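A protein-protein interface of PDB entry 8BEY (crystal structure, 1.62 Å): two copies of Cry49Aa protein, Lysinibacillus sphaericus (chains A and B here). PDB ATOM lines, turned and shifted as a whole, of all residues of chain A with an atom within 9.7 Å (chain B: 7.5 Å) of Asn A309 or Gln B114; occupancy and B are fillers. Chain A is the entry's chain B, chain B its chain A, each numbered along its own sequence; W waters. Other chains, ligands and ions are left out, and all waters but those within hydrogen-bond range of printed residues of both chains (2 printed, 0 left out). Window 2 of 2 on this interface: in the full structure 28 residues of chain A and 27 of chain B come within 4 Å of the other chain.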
ATOM      1  N   THR A 275     -37.306  -7.144  24.778  1.00  0.00           N
ATOM      2  CA  THR A 275     -37.465  -6.066  23.767  1.00  0.00           C
ATOM      3  C   THR A 275     -36.708  -6.478  22.506  1.00  0.00           C
ATOM      4  O   THR A 275     -35.885  -7.470  22.542  1.00  0.00           O
ATOM      5  CB  THR A 275     -37.028  -4.692  24.286  1.00  0.00           C
ATOM      6  OG1 THR A 275     -35.652  -4.804  24.673  1.00  0.00           O
ATOM      7  CG2 THR A 275     -37.846  -4.223  25.474  1.00  0.00           C
ATOM      8  N   ILE A 276     -36.969  -5.760  21.424  1.00  0.00           N
ATOM      9  CA  ILE A 276     -36.235  -5.950  20.144  1.00  0.00           C
ATOM     10  C   ILE A 276     -35.047  -4.996  20.159  1.00  0.00           C
ATOM     11  O   ILE A 276     -35.256  -3.739  20.247  1.00  0.00           O
ATOM     12  CB  ILE A 276     -37.163  -5.699  18.937  1.00  0.00           C
ATOM     13  CG1 ILE A 276     -38.471  -6.486  19.030  1.00  0.00           C
ATOM     14  CG2 ILE A 276     -36.407  -5.986  17.650  1.00  0.00           C
ATOM     15  CD1 ILE A 276     -38.277  -7.940  19.079  1.00  0.00           C
ATOM     16  N   GLY A 277     -33.820  -5.548  20.073  1.00  0.00           N
ATOM     17  CA  GLY A 277     -32.608  -4.712  19.996  1.00  0.00           C
ATOM     18  C   GLY A 277     -32.476  -4.001  18.663  1.00  0.00           C
ATOM     19  O   GLY A 277     -33.048  -4.479  17.612  1.00  0.00           O
ATOM     20  N   ALA A 278     -31.717  -2.896  18.667  1.00  0.00           N
ATOM     21  CA  ALA A 278     -31.557  -2.019  17.487  1.00  0.00           C
ATOM     22  C   ALA A 278     -30.760  -2.706  16.382  1.00  0.00           C
ATOM     23  O   ALA A 278     -30.771  -2.167  15.185  1.00  0.00           O
ATOM     24  CB  ALA A 278     -30.914  -0.724  17.889  1.00  0.00           C
ATOM     25  N   ASP A 279     -30.071  -3.821  16.687  1.00  0.00           N
ATOM     26  CA  ASP A 279     -29.208  -4.507  15.692  1.00  0.00           C
ATOM     27  C   ASP A 279     -30.016  -5.366  14.709  1.00  0.00           C
ATOM     28  O   ASP A 279     -29.414  -5.798  13.670  1.00  0.00           O
ATOM     29  CB  ASP A 279     -28.066  -5.287  16.346  1.00  0.00           C
ATOM     30  CG  ASP A 279     -28.409  -6.145  17.537  1.00  0.00           C
ATOM     31  OD1 ASP A 279     -29.560  -6.010  18.094  1.00  0.00           O
ATOM     32  OD2 ASP A 279     -27.499  -6.916  17.933  1.00  0.00           O
ATOM     33  N   LEU A 284     -33.295 -10.287  20.007  1.00  0.00           N
ATOM     34  CA  LEU A 284     -33.994 -10.128  21.306  1.00  0.00           C
ATOM     35  C   LEU A 284     -33.025  -9.716  22.407  1.00  0.00           C
ATOM     36  O   LEU A 284     -31.878 -10.312  22.522  1.00  0.00           O
ATOM     37  CB  LEU A 284     -34.720 -11.424  21.687  1.00  0.00           C
ATOM     38  CG  LEU A 284     -35.727 -11.979  20.684  1.00  0.00           C
ATOM     39  CD1 LEU A 284     -36.526 -13.117  21.296  1.00  0.00           C
ATOM     40  CD2 LEU A 284     -36.672 -10.920  20.173  1.00  0.00           C
ATOM     41  N   ARG A 285     -33.482  -8.745  23.208  1.00  0.00           N
ATOM     42  CA  ARG A 285     -32.847  -8.305  24.473  1.00  0.00           C
ATOM     43  C   ARG A 285     -33.664  -8.877  25.629  1.00  0.00           C
ATOM     44  O   ARG A 285     -34.944  -8.747  25.592  1.00  0.00           O
ATOM     45  CB  ARG A 285     -32.811  -6.781  24.564  1.00  0.00           C
ATOM     46  CG  ARG A 285     -31.885  -6.134  23.538  1.00  0.00           C
ATOM     47  CD  ARG A 285     -31.854  -4.629  23.748  1.00  0.00           C
ATOM     48  NE  ARG A 285     -31.086  -4.290  24.928  1.00  0.00           N
ATOM     49  CZ  ARG A 285     -31.191  -3.165  25.625  1.00  0.00           C
ATOM     50  NH1 ARG A 285     -32.030  -2.208  25.268  1.00  0.00           N
ATOM     51  NH2 ARG A 285     -30.408  -2.976  26.668  1.00  0.00           N
ATOM     52  N   PHE A 286     -32.986  -9.533  26.567  1.00  0.00           N
ATOM     53  CA  PHE A 286     -33.650 -10.187  27.719  1.00  0.00           C
ATOM     54  C   PHE A 286     -33.343  -9.407  28.993  1.00  0.00           C
ATOM     55  O   PHE A 286     -32.158  -8.953  29.220  1.00  0.00           O
ATOM     56  CB  PHE A 286     -33.177 -11.639  27.831  1.00  0.00           C
ATOM     57  CG  PHE A 286     -33.526 -12.492  26.645  1.00  0.00           C
ATOM     58  CD1 PHE A 286     -32.708 -12.522  25.523  1.00  0.00           C
ATOM     59  CD2 PHE A 286     -34.673 -13.278  26.659  1.00  0.00           C
ATOM     60  CE1 PHE A 286     -33.025 -13.326  24.437  1.00  0.00           C
ATOM     61  CE2 PHE A 286     -35.015 -14.053  25.554  1.00  0.00           C
ATOM     62  CZ  PHE A 286     -34.184 -14.080  24.444  1.00  0.00           C
ATOM     63  N   SER A 306     -29.608 -10.250  20.751  1.00  0.00           N
ATOM     64  CA  SER A 306     -29.142  -8.862  20.458  1.00  0.00           C
ATOM     65  C   SER A 306     -27.839  -8.583  21.197  1.00  0.00           C
ATOM     66  O   SER A 306     -27.669  -9.063  22.370  1.00  0.00           O
ATOM     67  CB  SER A 306     -30.201  -7.840  20.844  1.00  0.00           C
ATOM     68  OG  SER A 306     -29.724  -6.509  20.613  1.00  0.00           O
ATOM     69  N   PHE A 307     -26.929  -7.826  20.574  1.00  0.00           N
ATOM     70  CA  PHE A 307     -25.702  -7.313  21.242  1.00  0.00           C
ATOM     71  C   PHE A 307     -25.804  -5.806  21.499  1.00  0.00           C
ATOM     72  O   PHE A 307     -24.810  -5.236  21.996  1.00  0.00           O
ATOM     73  CB  PHE A 307     -24.459  -7.633  20.410  1.00  0.00           C
ATOM     74  CG  PHE A 307     -24.394  -9.062  19.946  1.00  0.00           C
ATOM     75  CD1 PHE A 307     -24.634 -10.099  20.828  1.00  0.00           C
ATOM     76  CD2 PHE A 307     -24.056  -9.369  18.637  1.00  0.00           C
ATOM     77  CE1 PHE A 307     -24.592 -11.420  20.398  1.00  0.00           C
ATOM     78  CE2 PHE A 307     -23.983 -10.690  18.220  1.00  0.00           C
ATOM     79  CZ  PHE A 307     -24.275 -11.704  19.090  1.00  0.00           C
ATOM     80  N   ALA A 308     -26.943  -5.185  21.178  1.00  0.00           N
ATOM     81  CA  ALA A 308     -27.123  -3.718  21.278  1.00  0.00           C
ATOM     82  C   ALA A 308     -27.505  -3.325  22.709  1.00  0.00           C
ATOM     83  O   ALA A 308     -28.148  -4.147  23.428  1.00  0.00           O
ATOM     84  CB  ALA A 308     -28.146  -3.251  20.267  1.00  0.00           C
ATOM     85  N   ASN A 309     -27.126  -2.095  23.091  1.00  0.00           N
ATOM     86  CA  ASN A 309     -27.581  -1.545  24.404  1.00  0.00           C
ATOM     87  C   ASN A 309     -28.707  -0.526  24.166  1.00  0.00           C
ATOM     88  O   ASN A 309     -29.086   0.173  25.125  1.00  0.00           O
ATOM     89  CB  ASN A 309     -26.435  -1.015  25.273  1.00  0.00           C
ATOM     90  CG  ASN A 309     -25.813  -2.116  26.106  1.00  0.00           C
ATOM     91  OD1 ASN A 309     -24.608  -2.331  26.054  1.00  0.00           O
ATOM     92  ND2 ASN A 309     -26.629  -2.842  26.851  1.00  0.00           N
ATOM     93  N   THR A 310     -29.274  -0.529  22.960  1.00  0.00           N
ATOM     94  CA  THR A 310     -30.382   0.360  22.525  1.00  0.00           C
ATOM     95  C   THR A 310     -31.505  -0.496  21.923  1.00  0.00           C
ATOM     96  O   THR A 310     -31.184  -1.512  21.222  1.00  0.00           O
ATOM     97  CB  THR A 310     -29.889   1.335  21.450  1.00  0.00           C
ATOM     98  OG1 THR A 310     -28.764   2.060  21.945  1.00  0.00           O
ATOM     99  CG2 THR A 310     -30.949   2.308  20.992  1.00  0.00           C
ATOM    100  N   ASN A 311     -32.763  -0.126  22.165  1.00  0.00           N
ATOM    101  CA  ASN A 311     -33.916  -0.813  21.532  1.00  0.00           C
ATOM    102  C   ASN A 311     -34.123  -0.286  20.118  1.00  0.00           C
ATOM    103  O   ASN A 311     -33.834   0.946  19.830  1.00  0.00           O
ATOM    104  CB  ASN A 311     -35.199  -0.652  22.343  1.00  0.00           C
ATOM    105  CG  ASN A 311     -35.140  -1.420  23.646  1.00  0.00           C
ATOM    106  OD1 ASN A 311     -34.478  -2.474  23.755  1.00  0.00           O
ATOM    107  ND2 ASN A 311     -35.822  -0.882  24.643  1.00  0.00           N
ATOM    108  N   TYR A 312     -34.617  -1.152  19.246  1.00  0.00           N
ATOM    109  CA  TYR A 312     -35.106  -0.755  17.902  1.00  0.00           C
ATOM    110  C   TYR A 312     -36.150   0.348  18.100  1.00  0.00           C
ATOM    111  O   TYR A 312     -37.061   0.233  18.997  1.00  0.00           O
ATOM    112  CB  TYR A 312     -35.669  -1.975  17.170  1.00  0.00           C
ATOM    113  CG  TYR A 312     -35.458  -2.012  15.683  1.00  0.00           C
ATOM    114  CD1 TYR A 312     -35.975  -1.015  14.855  1.00  0.00           C
ATOM    115  CD2 TYR A 312     -34.700  -3.014  15.094  1.00  0.00           C
ATOM    116  CE1 TYR A 312     -35.764  -1.042  13.475  1.00  0.00           C
ATOM    117  CE2 TYR A 312     -34.496  -3.062  13.722  1.00  0.00           C
ATOM    118  CZ  TYR A 312     -35.032  -2.074  12.908  1.00  0.00           C
ATOM    119  OH  TYR A 312     -34.755  -2.074  11.554  1.00  0.00           O
ATOM    120  N   ASN A 385     -33.101   7.086  17.232  1.00  0.00           N
ATOM    121  CA  ASN A 385     -31.713   6.878  17.723  1.00  0.00           C
ATOM    122  C   ASN A 385     -30.745   6.889  16.539  1.00  0.00           C
ATOM    123  O   ASN A 385     -31.209   6.976  15.344  1.00  0.00           O
ATOM    124  CB  ASN A 385     -31.616   5.611  18.583  1.00  0.00           C
ATOM    125  CG  ASN A 385     -31.886   4.342  17.805  1.00  0.00           C
ATOM    126  OD1 ASN A 385     -31.238   4.072  16.791  1.00  0.00           O
ATOM    127  ND2 ASN A 385     -32.883   3.572  18.232  1.00  0.00           N
ATOM    128  N   TYR A 387     -28.375   4.476  15.863  1.00  0.00           N
ATOM    129  CA  TYR A 387     -27.745   3.132  15.769  1.00  0.00           C
ATOM    130  C   TYR A 387     -27.470   2.776  14.303  1.00  0.00           C
ATOM    131  O   TYR A 387     -26.327   2.337  14.011  1.00  0.00           O
ATOM    132  CB  TYR A 387     -28.617   2.055  16.420  1.00  0.00           C
ATOM    133  CG  TYR A 387     -27.898   0.732  16.534  1.00  0.00           C
ATOM    134  CD1 TYR A 387     -27.897  -0.176  15.482  1.00  0.00           C
ATOM    135  CD2 TYR A 387     -27.190   0.408  17.674  1.00  0.00           C
ATOM    136  CE1 TYR A 387     -27.194  -1.372  15.562  1.00  0.00           C
ATOM    137  CE2 TYR A 387     -26.504  -0.796  17.776  1.00  0.00           C
ATOM    138  CZ  TYR A 387     -26.510  -1.690  16.716  1.00  0.00           C
ATOM    139  OH  TYR A 387     -25.798  -2.855  16.842  1.00  0.00           O
ATOM    140  N   PHE B 111     -16.114 -13.631  26.317  1.00  0.00           N
ATOM    141  CA  PHE B 111     -16.224 -12.226  25.863  1.00  0.00           C
ATOM    142  C   PHE B 111     -17.662 -11.884  25.505  1.00  0.00           C
ATOM    143  O   PHE B 111     -18.393 -12.724  24.892  1.00  0.00           O
ATOM    144  CB  PHE B 111     -15.265 -11.973  24.704  1.00  0.00           C
ATOM    145  CG  PHE B 111     -13.826 -12.003  25.124  1.00  0.00           C
ATOM    146  CD1 PHE B 111     -13.139 -13.205  25.203  1.00  0.00           C
ATOM    147  CD2 PHE B 111     -13.161 -10.829  25.483  1.00  0.00           C
ATOM    148  CE1 PHE B 111     -11.808 -13.230  25.606  1.00  0.00           C
ATOM    149  CE2 PHE B 111     -11.836 -10.867  25.895  1.00  0.00           C
ATOM    150  CZ  PHE B 111     -11.167 -12.067  25.953  1.00  0.00           C
ATOM    151  N   THR B 112     -18.048 -10.658  25.845  1.00  0.00           N
ATOM    152  CA  THR B 112     -19.358 -10.064  25.500  1.00  0.00           C
ATOM    153  C   THR B 112     -19.142  -9.069  24.360  1.00  0.00           C
ATOM    154  O   THR B 112     -18.245  -8.163  24.512  1.00  0.00           O
ATOM    155  CB  THR B 112     -20.006  -9.420  26.727  1.00  0.00           C
ATOM    156  OG1 THR B 112     -19.939 -10.360  27.803  1.00  0.00           O
ATOM    157  CG2 THR B 112     -21.438  -9.008  26.480  1.00  0.00           C
ATOM    158  N   ILE B 113     -19.915  -9.188  23.279  1.00  0.00           N
ATOM    159  CA  ILE B 113     -19.982  -8.120  22.237  1.00  0.00           C
ATOM    160  C   ILE B 113     -20.971  -7.062  22.713  1.00  0.00           C
ATOM    161  O   ILE B 113     -22.164  -7.405  23.002  1.00  0.00           O
ATOM    162  CB  ILE B 113     -20.360  -8.675  20.853  1.00  0.00           C
ATOM    163  CG1 ILE B 113     -19.410  -9.785  20.411  1.00  0.00           C
ATOM    164  CG2 ILE B 113     -20.437  -7.554  19.827  1.00  0.00           C
ATOM    165  CD1 ILE B 113     -19.851 -10.542  19.164  1.00  0.00           C
ATOM    166  N   GLN B 114     -20.515  -5.811  22.771  1.00  0.00           N
ATOM    167  CA  GLN B 114     -21.360  -4.638  23.052  1.00  0.00           C
ATOM    168  C   GLN B 114     -21.372  -3.796  21.766  1.00  0.00           C
ATOM    169  O   GLN B 114     -20.335  -3.118  21.466  1.00  0.00           O
ATOM    170  CB  GLN B 114     -20.788  -3.972  24.307  1.00  0.00           C
ATOM    171  CG  GLN B 114     -21.511  -2.742  24.799  1.00  0.00           C
ATOM    172  CD  GLN B 114     -20.682  -2.090  25.884  1.00  0.00           C
ATOM    173  OE1 GLN B 114     -20.163  -0.986  25.718  1.00  0.00           O
ATOM    174  NE2 GLN B 114     -20.489  -2.812  26.980  1.00  0.00           N
ATOM    175  N   SER B 115     -22.439  -3.892  20.975  1.00  0.00           N
ATOM    176  CA  SER B 115     -22.610  -3.122  19.719  1.00  0.00           C
ATOM    177  C   SER B 115     -23.056  -1.703  20.043  1.00  0.00           C
ATOM    178  O   SER B 115     -24.162  -1.530  20.606  1.00  0.00           O
ATOM    179  CB  SER B 115     -23.552  -3.801  18.765  1.00  0.00           C
ATOM    180  OG  SER B 115     -22.936  -4.989  18.316  1.00  0.00           O
ATOM    181  N   ILE B 116     -22.250  -0.721  19.619  1.00  0.00           N
ATOM    182  CA  ILE B 116     -22.490   0.744  19.772  1.00  0.00           C
ATOM    183  C   ILE B 116     -23.370   1.217  18.608  1.00  0.00           C
ATOM    184  O   ILE B 116     -24.241   2.086  18.832  1.00  0.00           O
ATOM    185  CB  ILE B 116     -21.145   1.515  19.809  1.00  0.00           C
ATOM    186  CG1 ILE B 116     -20.250   1.071  20.972  1.00  0.00           C
ATOM    187  CG2 ILE B 116     -21.371   3.009  19.820  1.00  0.00           C
ATOM    188  CD1 ILE B 116     -21.012   0.658  22.229  1.00  0.00           C
ATOM    189  N   ASN B 117     -23.099   0.692  17.415  1.00  0.00           N
ATOM    190  CA  ASN B 117     -23.891   0.946  16.193  1.00  0.00           C
ATOM    191  C   ASN B 117     -23.626  -0.196  15.207  1.00  0.00           C
ATOM    192  O   ASN B 117     -22.985  -1.214  15.620  1.00  0.00           O
ATOM    193  CB  ASN B 117     -23.601   2.344  15.643  1.00  0.00           C
ATOM    194  CG  ASN B 117     -22.182   2.476  15.152  1.00  0.00           C
ATOM    195  OD1 ASN B 117     -21.595   1.515  14.655  1.00  0.00           O
ATOM    196  ND2 ASN B 117     -21.613   3.646  15.308  1.00  0.00           N
ATOM    197  N   THR B 120     -19.752  -0.927  14.586  1.00  0.00           N
ATOM    198  CA  THR B 120     -18.819  -0.607  15.705  1.00  0.00           C
ATOM    199  C   THR B 120     -19.215  -1.376  16.959  1.00  0.00           C
ATOM    200  O   THR B 120     -20.420  -1.350  17.332  1.00  0.00           O
ATOM    201  CB  THR B 120     -18.775   0.895  16.018  1.00  0.00           C
ATOM    202  OG1 THR B 120     -18.571   1.574  14.780  1.00  0.00           O
ATOM    203  CG2 THR B 120     -17.682   1.278  16.989  1.00  0.00           C
ATOM    204  N   PHE B 121     -18.243  -2.012  17.605  1.00  0.00           N
ATOM    205  CA  PHE B 121     -18.485  -2.815  18.825  1.00  0.00           C
ATOM    206  C   PHE B 121     -17.307  -2.700  19.781  1.00  0.00           C
ATOM    207  O   PHE B 121     -16.183  -2.209  19.408  1.00  0.00           O
ATOM    208  CB  PHE B 121     -18.782  -4.276  18.465  1.00  0.00           C
ATOM    209  CG  PHE B 121     -17.619  -5.014  17.846  1.00  0.00           C
ATOM    210  CD1 PHE B 121     -17.393  -4.950  16.479  1.00  0.00           C
ATOM    211  CD2 PHE B 121     -16.736  -5.752  18.622  1.00  0.00           C
ATOM    212  CE1 PHE B 121     -16.303  -5.600  15.902  1.00  0.00           C
ATOM    213  CE2 PHE B 121     -15.646  -6.399  18.049  1.00  0.00           C
ATOM    214  CZ  PHE B 121     -15.421  -6.296  16.690  1.00  0.00           C
ATOM    215  N   ARG B 122     -17.554  -3.140  21.011  1.00  0.00           N
ATOM    216  CA  ARG B 122     -16.528  -3.291  22.062  1.00  0.00           C
ATOM    217  C   ARG B 122     -16.487  -4.752  22.492  1.00  0.00           C
ATOM    218  O   ARG B 122     -17.571  -5.457  22.428  1.00  0.00           O
ATOM    219  CB  ARG B 122     -16.826  -2.334  23.211  1.00  0.00           C
ATOM    220  CG  ARG B 122     -16.937  -0.889  22.762  1.00  0.00           C
ATOM    221  CD  ARG B 122     -17.599  -0.067  23.821  1.00  0.00           C
ATOM    222  NE  ARG B 122     -16.574   0.510  24.644  1.00  0.00           N
ATOM    223  CZ  ARG B 122     -16.664   0.750  25.949  1.00  0.00           C
ATOM    224  NH1 ARG B 122     -17.742   0.402  26.631  1.00  0.00           N
ATOM    225  NH2 ARG B 122     -15.650   1.331  26.568  1.00  0.00           N
ATOM    226  N   LEU B 123     -15.294  -5.220  22.871  1.00  0.00           N
ATOM    227  CA  LEU B 123     -15.103  -6.600  23.398  1.00  0.00           C
ATOM    228  C   LEU B 123     -14.947  -6.520  24.911  1.00  0.00           C
ATOM    229  O   LEU B 123     -13.848  -6.083  25.395  1.00  0.00           O
ATOM    230  CB  LEU B 123     -13.899  -7.267  22.743  1.00  0.00           C
ATOM    231  CG  LEU B 123     -14.135  -7.821  21.345  1.00  0.00           C
ATOM    232  CD1 LEU B 123     -12.849  -8.440  20.818  1.00  0.00           C
ATOM    233  CD2 LEU B 123     -15.287  -8.831  21.337  1.00  0.00           C
ATOM    234  N   HIS B 124     -15.996  -6.925  25.625  1.00  0.00           N
ATOM    235  CA  HIS B 124     -16.141  -6.770  27.089  1.00  0.00           C
ATOM    236  C   HIS B 124     -15.820  -8.087  27.801  1.00  0.00           C
ATOM    237  O   HIS B 124     -16.421  -9.160  27.430  1.00  0.00           O
ATOM    238  CB  HIS B 124     -17.544  -6.266  27.402  1.00  0.00           C
ATOM    239  CG  HIS B 124     -17.752  -5.877  28.821  1.00  0.00           C
ATOM    240  ND1 HIS B 124     -18.936  -6.134  29.485  1.00  0.00           N
ATOM    241  CD2 HIS B 124     -16.960  -5.213  29.695  1.00  0.00           C
ATOM    242  CE1 HIS B 124     -18.868  -5.630  30.709  1.00  0.00           C
ATOM    243  NE2 HIS B 124     -17.667  -5.061  30.863  1.00  0.00           N
ATOM    244  N   ASN B 129     -14.819  -6.242  34.083  1.00  0.00           N
ATOM    245  CA  ASN B 129     -15.410  -4.983  33.566  1.00  0.00           C
ATOM    246  C   ASN B 129     -14.371  -4.222  32.729  1.00  0.00           C
ATOM    247  O   ASN B 129     -14.261  -2.973  32.883  1.00  0.00           O
ATOM    248  CB  ASN B 129     -15.977  -4.124  34.697  1.00  0.00           C
ATOM    249  CG  ASN B 129     -16.966  -3.099  34.188  1.00  0.00           C
ATOM    250  OD1 ASN B 129     -17.500  -3.230  33.088  1.00  0.00           O
ATOM    251  ND2 ASN B 129     -17.237  -2.089  34.986  1.00  0.00           N
ATOM    252  N   PHE B 131     -12.336  -3.695  28.686  1.00  0.00           N
ATOM    253  CA  PHE B 131     -12.546  -3.615  27.218  1.00  0.00           C
ATOM    254  C   PHE B 131     -11.205  -3.702  26.489  1.00  0.00           C
ATOM    255  O   PHE B 131     -10.214  -2.988  26.865  1.00  0.00           O
ATOM    256  CB  PHE B 131     -13.296  -2.334  26.862  1.00  0.00           C
ATOM    257  CG  PHE B 131     -14.650  -2.227  27.511  1.00  0.00           C
ATOM    258  CD1 PHE B 131     -14.797  -1.645  28.761  1.00  0.00           C
ATOM    259  CD2 PHE B 131     -15.772  -2.761  26.894  1.00  0.00           C
ATOM    260  CE1 PHE B 131     -16.042  -1.581  29.372  1.00  0.00           C
ATOM    261  CE2 PHE B 131     -17.017  -2.689  27.503  1.00  0.00           C
ATOM    262  CZ  PHE B 131     -17.150  -2.097  28.739  1.00  0.00           C
ATOM    263  N   ASP B 150     -13.142   1.356  31.887  1.00  0.00           N
ATOM    264  CA  ASP B 150     -13.554   2.699  31.400  1.00  0.00           C
ATOM    265  C   ASP B 150     -13.156   3.739  32.448  1.00  0.00           C
ATOM    266  O   ASP B 150     -13.500   3.547  33.625  1.00  0.00           O
ATOM    267  CB  ASP B 150     -15.053   2.778  31.105  1.00  0.00           C
ATOM    268  CG  ASP B 150     -15.447   2.235  29.747  1.00  0.00           C
ATOM    269  OD1 ASP B 150     -14.539   1.973  28.916  1.00  0.00           O
ATOM    270  OD2 ASP B 150     -16.665   2.073  29.533  1.00  0.00           O
ATOM    271  N   ALA B 157     -11.919   2.166  23.051  1.00  0.00           N
ATOM    272  CA  ALA B 157     -12.053   0.697  22.898  1.00  0.00           C
ATOM    273  C   ALA B 157     -13.080   0.336  21.818  1.00  0.00           C
ATOM    274  O   ALA B 157     -13.594  -0.827  21.841  1.00  0.00           O
ATOM    275  CB  ALA B 157     -12.403   0.080  24.229  1.00  0.00           C
ATOM    276  N   ASN B 158     -13.365   1.251  20.892  1.00  0.00           N
ATOM    277  CA  ASN B 158     -14.317   1.009  19.776  1.00  0.00           C
ATOM    278  C   ASN B 158     -13.581   0.231  18.689  1.00  0.00           C
ATOM    279  O   ASN B 158     -12.462   0.650  18.286  1.00  0.00           O
ATOM    280  CB  ASN B 158     -14.949   2.299  19.251  1.00  0.00           C
ATOM    281  CG  ASN B 158     -15.903   2.925  20.242  1.00  0.00           C
ATOM    282  OD1 ASN B 158     -16.225   2.340  21.272  1.00  0.00           O
ATOM    283  ND2 ASN B 158     -16.398   4.097  19.908  1.00  0.00           N
ATOM    284  N   LEU B 159     -14.154  -0.910  18.298  1.00  0.00           N
ATOM    285  CA  LEU B 159     -13.567  -1.852  17.321  1.00  0.00           C
ATOM    286  C   LEU B 159     -14.505  -2.037  16.122  1.00  0.00           C
ATOM    287  O   LEU B 159     -15.764  -1.698  16.208  1.00  0.00           O
ATOM    288  CB  LEU B 159     -13.326  -3.210  17.989  1.00  0.00           C
ATOM    289  CG  LEU B 159     -12.549  -3.188  19.299  1.00  0.00           C
ATOM    290  CD1 LEU B 159     -12.504  -4.569  19.916  1.00  0.00           C
ATOM    291  CD2 LEU B 159     -11.136  -2.642  19.086  1.00  0.00           C
HETATM  292  O   HOH W   1     -25.018  -6.465  16.861  1.00  0.00           O
HETATM  293  O   HOH W   2     -26.266  -0.239  21.142  1.00  0.00           O
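Printed residues of chain B within 4 Å of Asn A309: Gln B114 (3.4 Å) and Ser B115 (3.9 Å). Printed residues of chain A within 4 Å of Ile B113: Phe A307 (3.5 Å). Printed residues of chain B within 4 Å of Phe A307: Ile B113 (3.5 Å), Gln B114 (3.7 Å) and Ser B115 (2.9 Å). Of the printed residues of chain A, Ile B116 touches Tyr A387. Asn A311 touches none of the printed residues of chain B. Phe B121 touches none of the printed residues of chain A. The nearest printed residue of chain A that does not touch Gln B114 is Ala A308 (5.8 Å). The nearest printed residue of chain A that does not touch Ser B115 is Asp A279 (5.0 Å).
O of Ala A308 sits at hydrogen-bond distance from NE of Arg A285, at 3.3 Å. The side-chain hydroxyl (OG1) of Thr B120 lies within hydrogen-bond range of the side-chain amide oxygen (OD1) of Asn B117, at 3.0 Å. The side-chain carboxylate (OD2) of Asp A279 sits at hydrogen-bond distance from the backbone NH (N) of Phe A307, at 2.9 Å. N of Tyr A387 is in hydrogen-bond range of OD1 of Asn A385, 3.0 Å away. The backbone NH of Ala A308 sits at hydrogen-bond distance from the side-chain hydroxyl of Ser A306, 3.1 Å away. N of Arg B122 is in hydrogen-bond range of O of Gln B114.
O of Asn B117 sits at hydrogen-bond distance from OH of Tyr A387, at 3.5 Å. The backbone carbonyl oxygen (O) of Phe A307 sits at hydrogen-bond distance from the backbone NH (N) of Ser B115.
Of the 18 printed residues of chain B, 5 touch a printed residue of chain A. Printed residues of chain B that touch a printed residue of chain A: Ile B113, Gln B114, Ser B115, Ile B116 and Asn B117. Of the 17 printed residues of chain A, 4 touch a printed residue of chain B. Hydrophobic or aromatic side chains of chain A within 4 Å of the printed part of chain B: Phe A307 and Tyr A387. Among the printed residues, no Asp or Glu carboxylate lies within 4 Å of a Lys or Arg side-chain nitrogen of the other chain.
Water W2 lies within hydrogen-bond range of O of Ser B115 (2.5 Å), N of Asn A309 (2.8 Å) and OG1 of Thr A310 (3.5 Å). Water W1 bridges OD2 of Asp A279 (2.7 Å) and OG of Ser B115 (2.9 Å).
No position is printed for both chains. Of the 9 pairs that touch across the chains among the printed residues, none has its exchanged pair printed and touching as well.
Among the printed residues, pairs that only touch across the chains: Tyr A387 with Ser B115 (3.1 Å), Asn A309 with Gln B114 (3.4 Å), Phe A307 with Ile B113 (3.5 Å), Tyr A387 with Ile B116 (3.6 Å), Phe A307 with Gln B114 (3.7 Å), Ala A308 with Ser B115 (3.7 Å) and Asn A309 with Ser B115 (3.9 Å).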
